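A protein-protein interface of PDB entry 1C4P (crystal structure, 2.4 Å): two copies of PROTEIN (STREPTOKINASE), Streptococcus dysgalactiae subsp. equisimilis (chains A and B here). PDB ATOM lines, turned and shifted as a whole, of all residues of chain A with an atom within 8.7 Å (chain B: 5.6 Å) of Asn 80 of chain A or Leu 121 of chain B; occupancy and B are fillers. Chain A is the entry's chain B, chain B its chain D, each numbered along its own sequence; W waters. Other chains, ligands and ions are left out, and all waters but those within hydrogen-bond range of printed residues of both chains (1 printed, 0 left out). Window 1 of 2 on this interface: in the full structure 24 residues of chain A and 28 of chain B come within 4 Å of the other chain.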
ATOM      1  N   THR A  77     -19.496   3.569  17.032  1.00  0.00           N
ATOM      2  CA  THR A  77     -19.548   3.120  15.657  1.00  0.00           C
ATOM      3  C   THR A  77     -20.582   1.986  15.739  1.00  0.00           C
ATOM      4  O   THR A  77     -20.460   1.090  16.565  1.00  0.00           O
ATOM      5  CB  THR A  77     -18.207   2.537  15.193  1.00  0.00           C
ATOM      6  OG1 THR A  77     -17.171   3.481  15.442  1.00  0.00           O
ATOM      7  CG2 THR A  77     -18.246   2.190  13.716  1.00  0.00           C
ATOM      8  N   HIS A  78     -21.598   2.053  14.886  1.00  0.00           N
ATOM      9  CA  HIS A  78     -22.658   1.046  14.838  1.00  0.00           C
ATOM     10  C   HIS A  78     -22.459   0.150  13.618  1.00  0.00           C
ATOM     11  O   HIS A  78     -22.220   0.641  12.521  1.00  0.00           O
ATOM     12  CB  HIS A  78     -24.039   1.710  14.715  1.00  0.00           C
ATOM     13  CG  HIS A  78     -24.208   2.947  15.548  1.00  0.00           C
ATOM     14  ND1 HIS A  78     -24.012   4.217  15.044  1.00  0.00           N
ATOM     15  CD2 HIS A  78     -24.548   3.109  16.852  1.00  0.00           C
ATOM     16  CE1 HIS A  78     -24.222   5.107  16.002  1.00  0.00           C
ATOM     17  NE2 HIS A  78     -24.548   4.459  17.108  1.00  0.00           N
ATOM     18  N   ASP A  79     -22.539  -1.158  13.820  1.00  0.00           N
ATOM     19  CA  ASP A  79     -22.444  -2.132  12.729  1.00  0.00           C
ATOM     20  C   ASP A  79     -21.882  -1.690  11.376  1.00  0.00           C
ATOM     21  O   ASP A  79     -22.648  -1.552  10.402  1.00  0.00           O
ATOM     22  CB  ASP A  79     -23.822  -2.686  12.421  1.00  0.00           C
ATOM     23  CG  ASP A  79     -24.463  -3.305  13.596  1.00  0.00           C
ATOM     24  OD1 ASP A  79     -24.083  -4.451  13.921  1.00  0.00           O
ATOM     25  OD2 ASP A  79     -25.341  -2.648  14.192  1.00  0.00           O
ATOM     26  N   ASN A  80     -20.584  -1.469  11.276  1.00  0.00           N
ATOM     27  CA  ASN A  80     -20.027  -1.121   9.965  1.00  0.00           C
ATOM     28  C   ASN A  80     -20.634   0.058   9.227  1.00  0.00           C
ATOM     29  O   ASN A  80     -20.324   0.258   8.066  1.00  0.00           O
ATOM     30  CB  ASN A  80     -20.066  -2.328   9.018  1.00  0.00           C
ATOM     31  CG  ASN A  80     -19.318  -3.515   9.557  1.00  0.00           C
ATOM     32  OD1 ASN A  80     -18.200  -3.384  10.043  1.00  0.00           O
ATOM     33  ND2 ASN A  80     -19.924  -4.697   9.463  1.00  0.00           N
ATOM     34  N   ASP A  81     -21.503   0.829   9.855  1.00  0.00           N
ATOM     35  CA  ASP A  81     -22.033   1.998   9.168  1.00  0.00           C
ATOM     36  C   ASP A  81     -20.933   3.063   9.223  1.00  0.00           C
ATOM     37  O   ASP A  81     -20.154   3.107  10.180  1.00  0.00           O
ATOM     38  CB  ASP A  81     -23.298   2.526   9.861  1.00  0.00           C
ATOM     39  CG  ASP A  81     -24.370   1.471   9.985  1.00  0.00           C
ATOM     40  OD1 ASP A  81     -24.267   0.451   9.263  1.00  0.00           O
ATOM     41  OD2 ASP A  81     -25.310   1.654  10.794  1.00  0.00           O
ATOM     42  N   ILE A  82     -20.882   3.927   8.213  1.00  0.00           N
ATOM     43  CA  ILE A  82     -19.874   4.989   8.140  1.00  0.00           C
ATOM     44  C   ILE A  82     -20.070   6.165   9.117  1.00  0.00           C
ATOM     45  O   ILE A  82     -19.106   6.772   9.578  1.00  0.00           O
ATOM     46  CB  ILE A  82     -19.779   5.508   6.679  1.00  0.00           C
ATOM     47  CG1 ILE A  82     -18.632   4.802   5.962  1.00  0.00           C
ATOM     48  CG2 ILE A  82     -19.556   7.005   6.631  1.00  0.00           C
ATOM     49  CD1 ILE A  82     -18.855   3.329   5.759  1.00  0.00           C
ATOM     50  N   PHE A  83     -21.317   6.481   9.441  1.00  0.00           N
ATOM     51  CA  PHE A  83     -21.588   7.593  10.349  1.00  0.00           C
ATOM     52  C   PHE A  83     -21.463   7.205  11.815  1.00  0.00           C
ATOM     53  O   PHE A  83     -22.248   6.402  12.307  1.00  0.00           O
ATOM     54  CB  PHE A  83     -22.994   8.151  10.109  1.00  0.00           C
ATOM     55  CG  PHE A  83     -23.192   8.771   8.754  1.00  0.00           C
ATOM     56  CD1 PHE A  83     -22.151   8.852   7.840  1.00  0.00           C
ATOM     57  CD2 PHE A  83     -24.441   9.276   8.392  1.00  0.00           C
ATOM     58  CE1 PHE A  83     -22.341   9.421   6.585  1.00  0.00           C
ATOM     59  CE2 PHE A  83     -24.637   9.846   7.141  1.00  0.00           C
ATOM     60  CZ  PHE A  83     -23.579   9.916   6.236  1.00  0.00           C
ATOM     61  N   ARG A  84     -20.475   7.776  12.499  1.00  0.00           N
ATOM     62  CA  ARG A  84     -20.245   7.510  13.930  1.00  0.00           C
ATOM     63  C   ARG A  84     -20.981   8.567  14.774  1.00  0.00           C
ATOM     64  O   ARG A  84     -21.289   9.673  14.291  1.00  0.00           O
ATOM     65  CB  ARG A  84     -18.742   7.565  14.258  1.00  0.00           C
ATOM     66  CG  ARG A  84     -17.892   6.561  13.520  1.00  0.00           C
ATOM     67  CD  ARG A  84     -16.407   6.895  13.564  1.00  0.00           C
ATOM     68  NE  ARG A  84     -16.106   8.105  12.808  1.00  0.00           N
ATOM     69  CZ  ARG A  84     -14.877   8.553  12.539  1.00  0.00           C
ATOM     70  NH1 ARG A  84     -13.800   7.898  12.967  1.00  0.00           N
ATOM     71  NH2 ARG A  84     -14.723   9.673  11.832  1.00  0.00           N
ATOM     72  N   ARG A 100     -31.850   0.127  14.520  1.00  0.00           N
ATOM     73  CA  ARG A 100     -31.260  -0.291  13.253  1.00  0.00           C
ATOM     74  C   ARG A 100     -31.834  -1.622  12.755  1.00  0.00           C
ATOM     75  O   ARG A 100     -32.573  -2.298  13.459  1.00  0.00           O
ATOM     76  CB  ARG A 100     -29.746  -0.438  13.421  1.00  0.00           C
ATOM     77  CG  ARG A 100     -29.368  -1.661  14.252  1.00  0.00           C
ATOM     78  CD  ARG A 100     -28.029  -1.504  14.977  1.00  0.00           C
ATOM     79  NE  ARG A 100     -28.087  -0.568  16.101  1.00  0.00           N
ATOM     80  CZ  ARG A 100     -27.088  -0.361  16.961  1.00  0.00           C
ATOM     81  NH1 ARG A 100     -25.949  -1.021  16.837  1.00  0.00           N
ATOM     82  NH2 ARG A 100     -27.222   0.515  17.946  1.00  0.00           N
ATOM     83  N   ALA A 103     -29.111  -7.544  12.201  1.00  0.00           N
ATOM     84  CA  ALA A 103     -27.885  -8.014  11.573  1.00  0.00           C
ATOM     85  C   ALA A 103     -28.050  -9.495  11.269  1.00  0.00           C
ATOM     86  O   ALA A 103     -28.780 -10.191  11.968  1.00  0.00           O
ATOM     87  CB  ALA A 103     -26.691  -7.791  12.509  1.00  0.00           C
ATOM     88  N   TYR A 104     -27.383  -9.976  10.226  1.00  0.00           N
ATOM     89  CA  TYR A 104     -27.479 -11.380   9.871  1.00  0.00           C
ATOM     90  C   TYR A 104     -26.338 -11.768   8.958  1.00  0.00           C
ATOM     91  O   TYR A 104     -25.797 -10.935   8.247  1.00  0.00           O
ATOM     92  CB  TYR A 104     -28.822 -11.662   9.187  1.00  0.00           C
ATOM     93  CG  TYR A 104     -28.933 -11.081   7.802  1.00  0.00           C
ATOM     94  CD1 TYR A 104     -28.482 -11.792   6.692  1.00  0.00           C
ATOM     95  CD2 TYR A 104     -29.491  -9.819   7.600  1.00  0.00           C
ATOM     96  CE1 TYR A 104     -28.590 -11.264   5.402  1.00  0.00           C
ATOM     97  CE2 TYR A 104     -29.600  -9.275   6.317  1.00  0.00           C
ATOM     98  CZ  TYR A 104     -29.151 -10.008   5.222  1.00  0.00           C
ATOM     99  OH  TYR A 104     -29.273  -9.492   3.958  1.00  0.00           O
ATOM    100  N   GLU A 105     -25.979 -13.043   8.982  1.00  0.00           N
ATOM    101  CA  GLU A 105     -24.894 -13.541   8.156  1.00  0.00           C
ATOM    102  C   GLU A 105     -25.318 -14.697   7.278  1.00  0.00           C
ATOM    103  O   GLU A 105     -26.500 -14.944   7.061  1.00  0.00           O
ATOM    104  CB  GLU A 105     -23.755 -14.032   9.027  1.00  0.00           C
ATOM    105  CG  GLU A 105     -23.047 -12.977   9.793  1.00  0.00           C
ATOM    106  CD  GLU A 105     -21.868 -13.547  10.540  1.00  0.00           C
ATOM    107  OE1 GLU A 105     -22.065 -14.561  11.256  1.00  0.00           O
ATOM    108  OE2 GLU A 105     -20.753 -12.984  10.409  1.00  0.00           O
ATOM    109  N   ILE A 116     -27.584 -12.664  13.725  1.00  0.00           N
ATOM    110  CA  ILE A 116     -26.483 -12.547  14.682  1.00  0.00           C
ATOM    111  C   ILE A 116     -26.721 -11.258  15.418  1.00  0.00           C
ATOM    112  O   ILE A 116     -27.517 -10.436  14.980  1.00  0.00           O
ATOM    113  CB  ILE A 116     -25.117 -12.415  13.993  1.00  0.00           C
ATOM    114  CG1 ILE A 116     -25.226 -11.419  12.839  1.00  0.00           C
ATOM    115  CG2 ILE A 116     -24.617 -13.782  13.535  1.00  0.00           C
ATOM    116  CD1 ILE A 116     -23.901 -11.082  12.233  1.00  0.00           C
ATOM    117  N   ASN A 118     -26.270  -7.467  16.630  1.00  0.00           N
ATOM    118  CA  ASN A 118     -25.721  -6.251  16.064  1.00  0.00           C
ATOM    119  C   ASN A 118     -24.600  -5.784  17.002  1.00  0.00           C
ATOM    120  O   ASN A 118     -24.422  -6.340  18.088  1.00  0.00           O
ATOM    121  CB  ASN A 118     -26.805  -5.192  15.940  1.00  0.00           C
ATOM    122  CG  ASN A 118     -27.679  -5.423  14.741  1.00  0.00           C
ATOM    123  OD1 ASN A 118     -27.752  -4.585  13.843  1.00  0.00           O
ATOM    124  ND2 ASN A 118     -28.335  -6.577  14.703  1.00  0.00           N
ATOM    125  N   THR A 119     -23.845  -4.775  16.589  1.00  0.00           N
ATOM    126  CA  THR A 119     -22.727  -4.289  17.384  1.00  0.00           C
ATOM    127  C   THR A 119     -22.600  -2.774  17.511  1.00  0.00           C
ATOM    128  O   THR A 119     -22.773  -2.031  16.553  1.00  0.00           O
ATOM    129  CB  THR A 119     -21.389  -4.815  16.808  1.00  0.00           C
ATOM    130  OG1 THR A 119     -21.310  -6.232  16.989  1.00  0.00           O
ATOM    131  CG2 THR A 119     -20.204  -4.164  17.502  1.00  0.00           C
ATOM    132  N   ASP A 120     -22.309  -2.336  18.724  1.00  0.00           N
ATOM    133  CA  ASP A 120     -22.055  -0.936  19.010  1.00  0.00           C
ATOM    134  C   ASP A 120     -20.666  -1.016  19.622  1.00  0.00           C
ATOM    135  O   ASP A 120     -20.392  -1.903  20.419  1.00  0.00           O
ATOM    136  CB  ASP A 120     -23.042  -0.345  20.048  1.00  0.00           C
ATOM    137  CG  ASP A 120     -24.181   0.430  19.401  1.00  0.00           C
ATOM    138  OD1 ASP A 120     -24.090   0.692  18.182  1.00  0.00           O
ATOM    139  OD2 ASP A 120     -25.158   0.780  20.100  1.00  0.00           O
ATOM    140  N   LEU A 121     -19.778  -0.127  19.214  1.00  0.00           N
ATOM    141  CA  LEU A 121     -18.422  -0.087  19.754  1.00  0.00           C
ATOM    142  C   LEU A 121     -18.235   1.300  20.320  1.00  0.00           C
ATOM    143  O   LEU A 121     -18.156   2.261  19.590  1.00  0.00           O
ATOM    144  CB  LEU A 121     -17.385  -0.333  18.656  1.00  0.00           C
ATOM    145  CG  LEU A 121     -15.920  -0.101  19.065  1.00  0.00           C
ATOM    146  CD1 LEU A 121     -15.513  -0.936  20.280  1.00  0.00           C
ATOM    147  CD2 LEU A 121     -15.029  -0.457  17.853  1.00  0.00           C
ATOM    148  N   ASP B  11      -3.904  -6.373   8.936  1.00  0.00           N
ATOM    149  CA  ASP B  11      -4.987  -7.209   8.443  1.00  0.00           C
ATOM    150  C   ASP B  11      -5.928  -6.247   7.767  1.00  0.00           C
ATOM    151  O   ASP B  11      -6.569  -5.399   8.421  1.00  0.00           O
ATOM    152  CB  ASP B  11      -5.714  -7.931   9.586  1.00  0.00           C
ATOM    153  CG  ASP B  11      -4.908  -9.104  10.149  1.00  0.00           C
ATOM    154  OD1 ASP B  11      -4.180  -9.748   9.369  1.00  0.00           O
ATOM    155  OD2 ASP B  11      -5.007  -9.400  11.362  1.00  0.00           O
ATOM    156  N   GLU B  13      -9.212  -5.524   6.309  1.00  0.00           N
ATOM    157  CA  GLU B  13     -10.581  -6.017   6.300  1.00  0.00           C
ATOM    158  C   GLU B  13     -11.501  -5.274   5.332  1.00  0.00           C
ATOM    159  O   GLU B  13     -11.340  -4.071   5.086  1.00  0.00           O
ATOM    160  CB  GLU B  13     -11.142  -5.954   7.700  1.00  0.00           C
ATOM    161  CG  GLU B  13     -11.317  -7.305   8.288  1.00  0.00           C
ATOM    162  CD  GLU B  13     -11.073  -7.304   9.758  1.00  0.00           C
ATOM    163  OE1 GLU B  13     -11.780  -6.523  10.456  1.00  0.00           O
ATOM    164  OE2 GLU B  13     -10.181  -8.077  10.202  1.00  0.00           O
ATOM    165  N   TYR B  14     -12.465  -5.997   4.775  1.00  0.00           N
ATOM    166  CA  TYR B  14     -13.389  -5.391   3.827  1.00  0.00           C
ATOM    167  C   TYR B  14     -14.850  -5.653   4.163  1.00  0.00           C
ATOM    168  O   TYR B  14     -15.247  -6.776   4.484  1.00  0.00           O
ATOM    169  CB  TYR B  14     -13.088  -5.881   2.407  1.00  0.00           C
ATOM    170  CG  TYR B  14     -13.917  -5.210   1.341  1.00  0.00           C
ATOM    171  CD1 TYR B  14     -13.592  -3.927   0.852  1.00  0.00           C
ATOM    172  CD2 TYR B  14     -15.042  -5.843   0.831  1.00  0.00           C
ATOM    173  CE1 TYR B  14     -14.385  -3.308  -0.121  1.00  0.00           C
ATOM    174  CE2 TYR B  14     -15.829  -5.244  -0.129  1.00  0.00           C
ATOM    175  CZ  TYR B  14     -15.512  -3.990  -0.605  1.00  0.00           C
ATOM    176  OH  TYR B  14     -16.357  -3.442  -1.541  1.00  0.00           O
ATOM    177  N   THR B  15     -15.648  -4.592   4.079  1.00  0.00           N
ATOM    178  CA  THR B  15     -17.067  -4.663   4.371  1.00  0.00           C
ATOM    179  C   THR B  15     -17.745  -3.770   3.359  1.00  0.00           C
ATOM    180  O   THR B  15     -17.254  -2.686   3.069  1.00  0.00           O
ATOM    181  CB  THR B  15     -17.365  -4.163   5.813  1.00  0.00           C
ATOM    182  OG1 THR B  15     -18.722  -4.466   6.158  1.00  0.00           O
ATOM    183  CG2 THR B  15     -17.147  -2.667   5.929  1.00  0.00           C
ATOM    184  N   GLN B  17     -21.698  -2.205   1.994  1.00  0.00           N
ATOM    185  CA  GLN B  17     -23.120  -1.988   2.266  1.00  0.00           C
ATOM    186  C   GLN B  17     -23.794  -1.625   0.956  1.00  0.00           C
ATOM    187  O   GLN B  17     -23.351  -0.715   0.267  1.00  0.00           O
ATOM    188  CB  GLN B  17     -23.299  -0.830   3.252  1.00  0.00           C
ATOM    189  CG  GLN B  17     -24.756  -0.359   3.456  1.00  0.00           C
ATOM    190  CD  GLN B  17     -24.842   0.985   4.198  1.00  0.00           C
ATOM    191  OE1 GLN B  17     -24.364   1.120   5.332  1.00  0.00           O
ATOM    192  NE2 GLN B  17     -25.447   1.988   3.551  1.00  0.00           N
ATOM    193  N   LYS B  32     -24.221  -8.565   7.405  1.00  0.00           N
ATOM    194  CA  LYS B  32     -22.845  -8.361   7.875  1.00  0.00           C
ATOM    195  C   LYS B  32     -21.970  -9.243   6.993  1.00  0.00           C
ATOM    196  O   LYS B  32     -22.131 -10.469   6.959  1.00  0.00           O
ATOM    197  CB  LYS B  32     -22.675  -8.763   9.344  1.00  0.00           C
ATOM    198  CG  LYS B  32     -21.218  -8.778   9.794  1.00  0.00           C
ATOM    199  CD  LYS B  32     -21.095  -9.171  11.238  1.00  0.00           C
ATOM    200  CE  LYS B  32     -19.652  -9.114  11.723  1.00  0.00           C
ATOM    201  NZ  LYS B  32     -19.581  -9.143  13.226  1.00  0.00           N
ATOM    202  N   ASP B  33     -21.041  -8.613   6.287  1.00  0.00           N
ATOM    203  CA  ASP B  33     -20.189  -9.332   5.360  1.00  0.00           C
ATOM    204  C   ASP B  33     -18.700  -9.053   5.519  1.00  0.00           C
ATOM    205  O   ASP B  33     -17.932  -9.308   4.595  1.00  0.00           O
ATOM    206  CB  ASP B  33     -20.605  -8.955   3.938  1.00  0.00           C
ATOM    207  CG  ASP B  33     -20.617  -7.428   3.719  1.00  0.00           C
ATOM    208  OD1 ASP B  33     -19.866  -6.713   4.427  1.00  0.00           O
ATOM    209  OD2 ASP B  33     -21.365  -6.947   2.841  1.00  0.00           O
ATOM    210  N   THR B  34     -18.281  -8.534   6.666  1.00  0.00           N
ATOM    211  CA  THR B  34     -16.872  -8.225   6.841  1.00  0.00           C
ATOM    212  C   THR B  34     -16.010  -9.443   6.612  1.00  0.00           C
ATOM    213  O   THR B  34     -16.183 -10.473   7.263  1.00  0.00           O
ATOM    214  CB  THR B  34     -16.586  -7.662   8.214  1.00  0.00           C
ATOM    215  OG1 THR B  34     -17.548  -6.647   8.496  1.00  0.00           O
ATOM    216  CG2 THR B  34     -15.201  -7.024   8.246  1.00  0.00           C
ATOM    217  N   ILE B  75     -14.239   4.218   2.292  1.00  0.00           N
ATOM    218  CA  ILE B  75     -13.635   4.757   3.515  1.00  0.00           C
ATOM    219  C   ILE B  75     -12.668   3.740   4.132  1.00  0.00           C
ATOM    220  O   ILE B  75     -12.865   2.536   3.987  1.00  0.00           O
ATOM    221  CB  ILE B  75     -14.794   5.071   4.532  1.00  0.00           C
ATOM    222  CG1 ILE B  75     -15.572   6.299   4.060  1.00  0.00           C
ATOM    223  CG2 ILE B  75     -14.279   5.264   5.928  1.00  0.00           C
ATOM    224  CD1 ILE B  75     -14.715   7.482   3.870  1.00  0.00           C
ATOM    225  N   VAL B  76     -11.617   4.215   4.793  1.00  0.00           N
ATOM    226  CA  VAL B  76     -10.680   3.300   5.453  1.00  0.00           C
ATOM    227  C   VAL B  76     -10.505   3.677   6.936  1.00  0.00           C
ATOM    228  O   VAL B  76     -10.081   4.791   7.265  1.00  0.00           O
ATOM    229  CB  VAL B  76      -9.262   3.268   4.787  1.00  0.00           C
ATOM    230  CG1 VAL B  76      -8.426   2.175   5.455  1.00  0.00           C
ATOM    231  CG2 VAL B  76      -9.357   3.002   3.297  1.00  0.00           C
ATOM    232  N   THR B  77     -10.842   2.748   7.825  1.00  0.00           N
ATOM    233  CA  THR B  77     -10.712   2.998   9.257  1.00  0.00           C
ATOM    234  C   THR B  77      -9.435   2.294   9.750  1.00  0.00           C
ATOM    235  O   THR B  77      -9.276   1.082   9.582  1.00  0.00           O
ATOM    236  CB  THR B  77     -11.950   2.469  10.000  1.00  0.00           C
ATOM    237  OG1 THR B  77     -13.127   3.005   9.384  1.00  0.00           O
ATOM    238  CG2 THR B  77     -11.927   2.886  11.460  1.00  0.00           C
ATOM    239  N   HIS B  78      -8.524   3.056  10.352  1.00  0.00           N
ATOM    240  CA  HIS B  78      -7.252   2.478  10.806  1.00  0.00           C
ATOM    241  C   HIS B  78      -7.213   2.176  12.293  1.00  0.00           C
ATOM    242  O   HIS B  78      -7.270   3.101  13.091  1.00  0.00           O
ATOM    243  CB  HIS B  78      -6.091   3.428  10.468  1.00  0.00           C
ATOM    244  CG  HIS B  78      -6.140   3.971   9.071  1.00  0.00           C
ATOM    245  ND1 HIS B  78      -6.541   5.263   8.787  1.00  0.00           N
ATOM    246  CD2 HIS B  78      -5.813   3.406   7.882  1.00  0.00           C
ATOM    247  CE1 HIS B  78      -6.454   5.470   7.485  1.00  0.00           C
ATOM    248  NE2 HIS B  78      -6.015   4.360   6.913  1.00  0.00           N
ATOM    249  N   THR B 119      -4.927  -3.373  12.295  1.00  0.00           N
ATOM    250  CA  THR B 119      -6.095  -3.574  11.450  1.00  0.00           C
ATOM    251  C   THR B 119      -6.476  -2.380  10.609  1.00  0.00           C
ATOM    252  O   THR B 119      -6.352  -1.229  11.022  1.00  0.00           O
ATOM    253  CB  THR B 119      -7.362  -3.957  12.288  1.00  0.00           C
ATOM    254  OG1 THR B 119      -7.058  -5.053  13.150  1.00  0.00           O
ATOM    255  CG2 THR B 119      -8.525  -4.384  11.366  1.00  0.00           C
ATOM    256  N   ASP B 120      -6.944  -2.680   9.408  1.00  0.00           N
ATOM    257  CA  ASP B 120      -7.444  -1.671   8.487  1.00  0.00           C
ATOM    258  C   ASP B 120      -8.862  -2.155   8.147  1.00  0.00           C
ATOM    259  O   ASP B 120      -9.084  -3.354   7.939  1.00  0.00           O
ATOM    260  CB  ASP B 120      -6.604  -1.624   7.212  1.00  0.00           C
ATOM    261  CG  ASP B 120      -5.775  -0.341   7.094  1.00  0.00           C
ATOM    262  OD1 ASP B 120      -5.954   0.560   7.938  1.00  0.00           O
ATOM    263  OD2 ASP B 120      -4.948  -0.224   6.155  1.00  0.00           O
ATOM    264  N   LEU B 121      -9.837  -1.262   8.146  1.00  0.00           N
ATOM    265  CA  LEU B 121     -11.173  -1.679   7.743  1.00  0.00           C
ATOM    266  C   LEU B 121     -11.530  -0.774   6.569  1.00  0.00           C
ATOM    267  O   LEU B 121     -11.577   0.453   6.703  1.00  0.00           O
ATOM    268  CB  LEU B 121     -12.221  -1.548   8.882  1.00  0.00           C
ATOM    269  CG  LEU B 121     -13.679  -1.864   8.440  1.00  0.00           C
ATOM    270  CD1 LEU B 121     -13.709  -3.273   7.801  1.00  0.00           C
ATOM    271  CD2 LEU B 121     -14.670  -1.813   9.613  1.00  0.00           C
ATOM    272  N   ILE B 122     -11.744  -1.384   5.412  1.00  0.00           N
ATOM    273  CA  ILE B 122     -12.090  -0.649   4.215  1.00  0.00           C
ATOM    274  C   ILE B 122     -13.555  -0.865   4.043  1.00  0.00           C
ATOM    275  O   ILE B 122     -13.971  -1.984   3.810  1.00  0.00           O
ATOM    276  CB  ILE B 122     -11.353  -1.202   2.964  1.00  0.00           C
ATOM    277  CG1 ILE B 122      -9.837  -1.214   3.214  1.00  0.00           C
ATOM    278  CG2 ILE B 122     -11.685  -0.361   1.725  1.00  0.00           C
ATOM    279  CD1 ILE B 122      -9.029  -1.732   2.025  1.00  0.00           C
ATOM    280  N   SER B 123     -14.328   0.210   4.176  1.00  0.00           N
ATOM    281  CA  SER B 123     -15.793   0.187   4.065  1.00  0.00           C
ATOM    282  C   SER B 123     -16.282   0.871   2.794  1.00  0.00           C
ATOM    283  O   SER B 123     -15.894   2.014   2.477  1.00  0.00           O
ATOM    284  CB  SER B 123     -16.418   0.911   5.252  1.00  0.00           C
ATOM    285  OG  SER B 123     -15.771   0.555   6.448  1.00  0.00           O
HETATM  286  O   HOH W   1     -21.147  -5.558   6.783  1.00  0.00           O
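O of Tyr 104 of chain A sits at hydrogen-bond distance from N of Lys 32 of chain B (3.0 Å).
The side-chain amide nitrogen (ND2) of Asn 80 of chain A sits at hydrogen-bond distance from the side-chain hydroxyl (OG1) of Thr 34 of chain B, at 3.2 Å.
O of Leu 121 of chain B is in hydrogen-bond range of N of Thr 77 of chain B, at 2.7 Å.
N of Thr 15 of chain B lies within hydrogen-bond range of O of Ile 122 of chain B, at 3.1 Å.
OD1 of Asp 33 of chain B is in hydrogen-bond range of OG1 of Thr 15 of chain B.
The backbone carbonyl oxygen (O) of Ala 103 of chain A sits at hydrogen-bond distance from the backbone NH (N) of Ile 116 of chain A (3.3 Å).
The backbone carbonyl oxygen of Ile 75 of chain B sits at hydrogen-bond distance from the backbone NH of Ser 123 of chain B, at 2.8 Å.
The side-chain hydroxyl of Thr 34 of chain B lies within hydrogen-bond range of the side-chain hydroxyl of Thr 15 of chain B, 3.4 Å away.
Among the printed residues, merely in contact across the chains: Asn 80 of chain A with Thr 15 of chain B (3.5 Å), Asn 80 of chain A with Leu 121 of chain B (3.9 Å), Asp 81 of chain A with Gln 17 of chain B (3.99 Å), Ile 82 of chain A with Ile 75 of chain B (3.9 Å), Ile 82 of chain A with Ser 123 of chain B (3.5 Å), Glu 105 of chain A with Lys 32 of chain B (3.9 Å) and Ile 116 of chain A with Lys 32 of chain B (3.5 Å).
Of chain B, only Thr 15 (3.5 Å), Thr 34 (3.2 Å) and Leu 121 (3.9 Å) come within 4 Å of Asn 80 of chain A.
Of the printed residues of chain A, Leu 121 of chain B touches Asn 80 (3.9 Å).
Printed residues of chain B within 4 Å of Ile 116 of chain A: Lys 32.
Of the printed residues of chain B, Ile 82 of chain A touches Ile 75 and Ser 123.
Printed residues of chain B within 4 Å of Glu 105 of chain A: Lys 32.
Of the printed residues of chain A, Gln 17 of chain B touches Asp 81 (3.99 Å).
Of the 17 printed residues of chain A, 6 touch a printed residue of chain B.
Of the 17 printed residues of chain B, 7 touch a printed residue of chain A.
Hydrophobic or aromatic side chains of chain B that line the printed part of chain A: Ile 75 and Leu 121.
Among the printed residues, 9 pairs touch across the chains.
5 positions are printed for both chains.
Of the 9 pairs that touch across the chains among the printed residues, none has its exchanged pair printed and touching as well.
Water W1 lies within hydrogen-bond range of the side-chain hydroxyl of Thr 15 of chain B (2.7 Å), the side-chain carboxylate of Asp 33 of chain B (2.9 Å) and the side-chain amide nitrogen of Asn 80 of chain A (3.1 Å).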
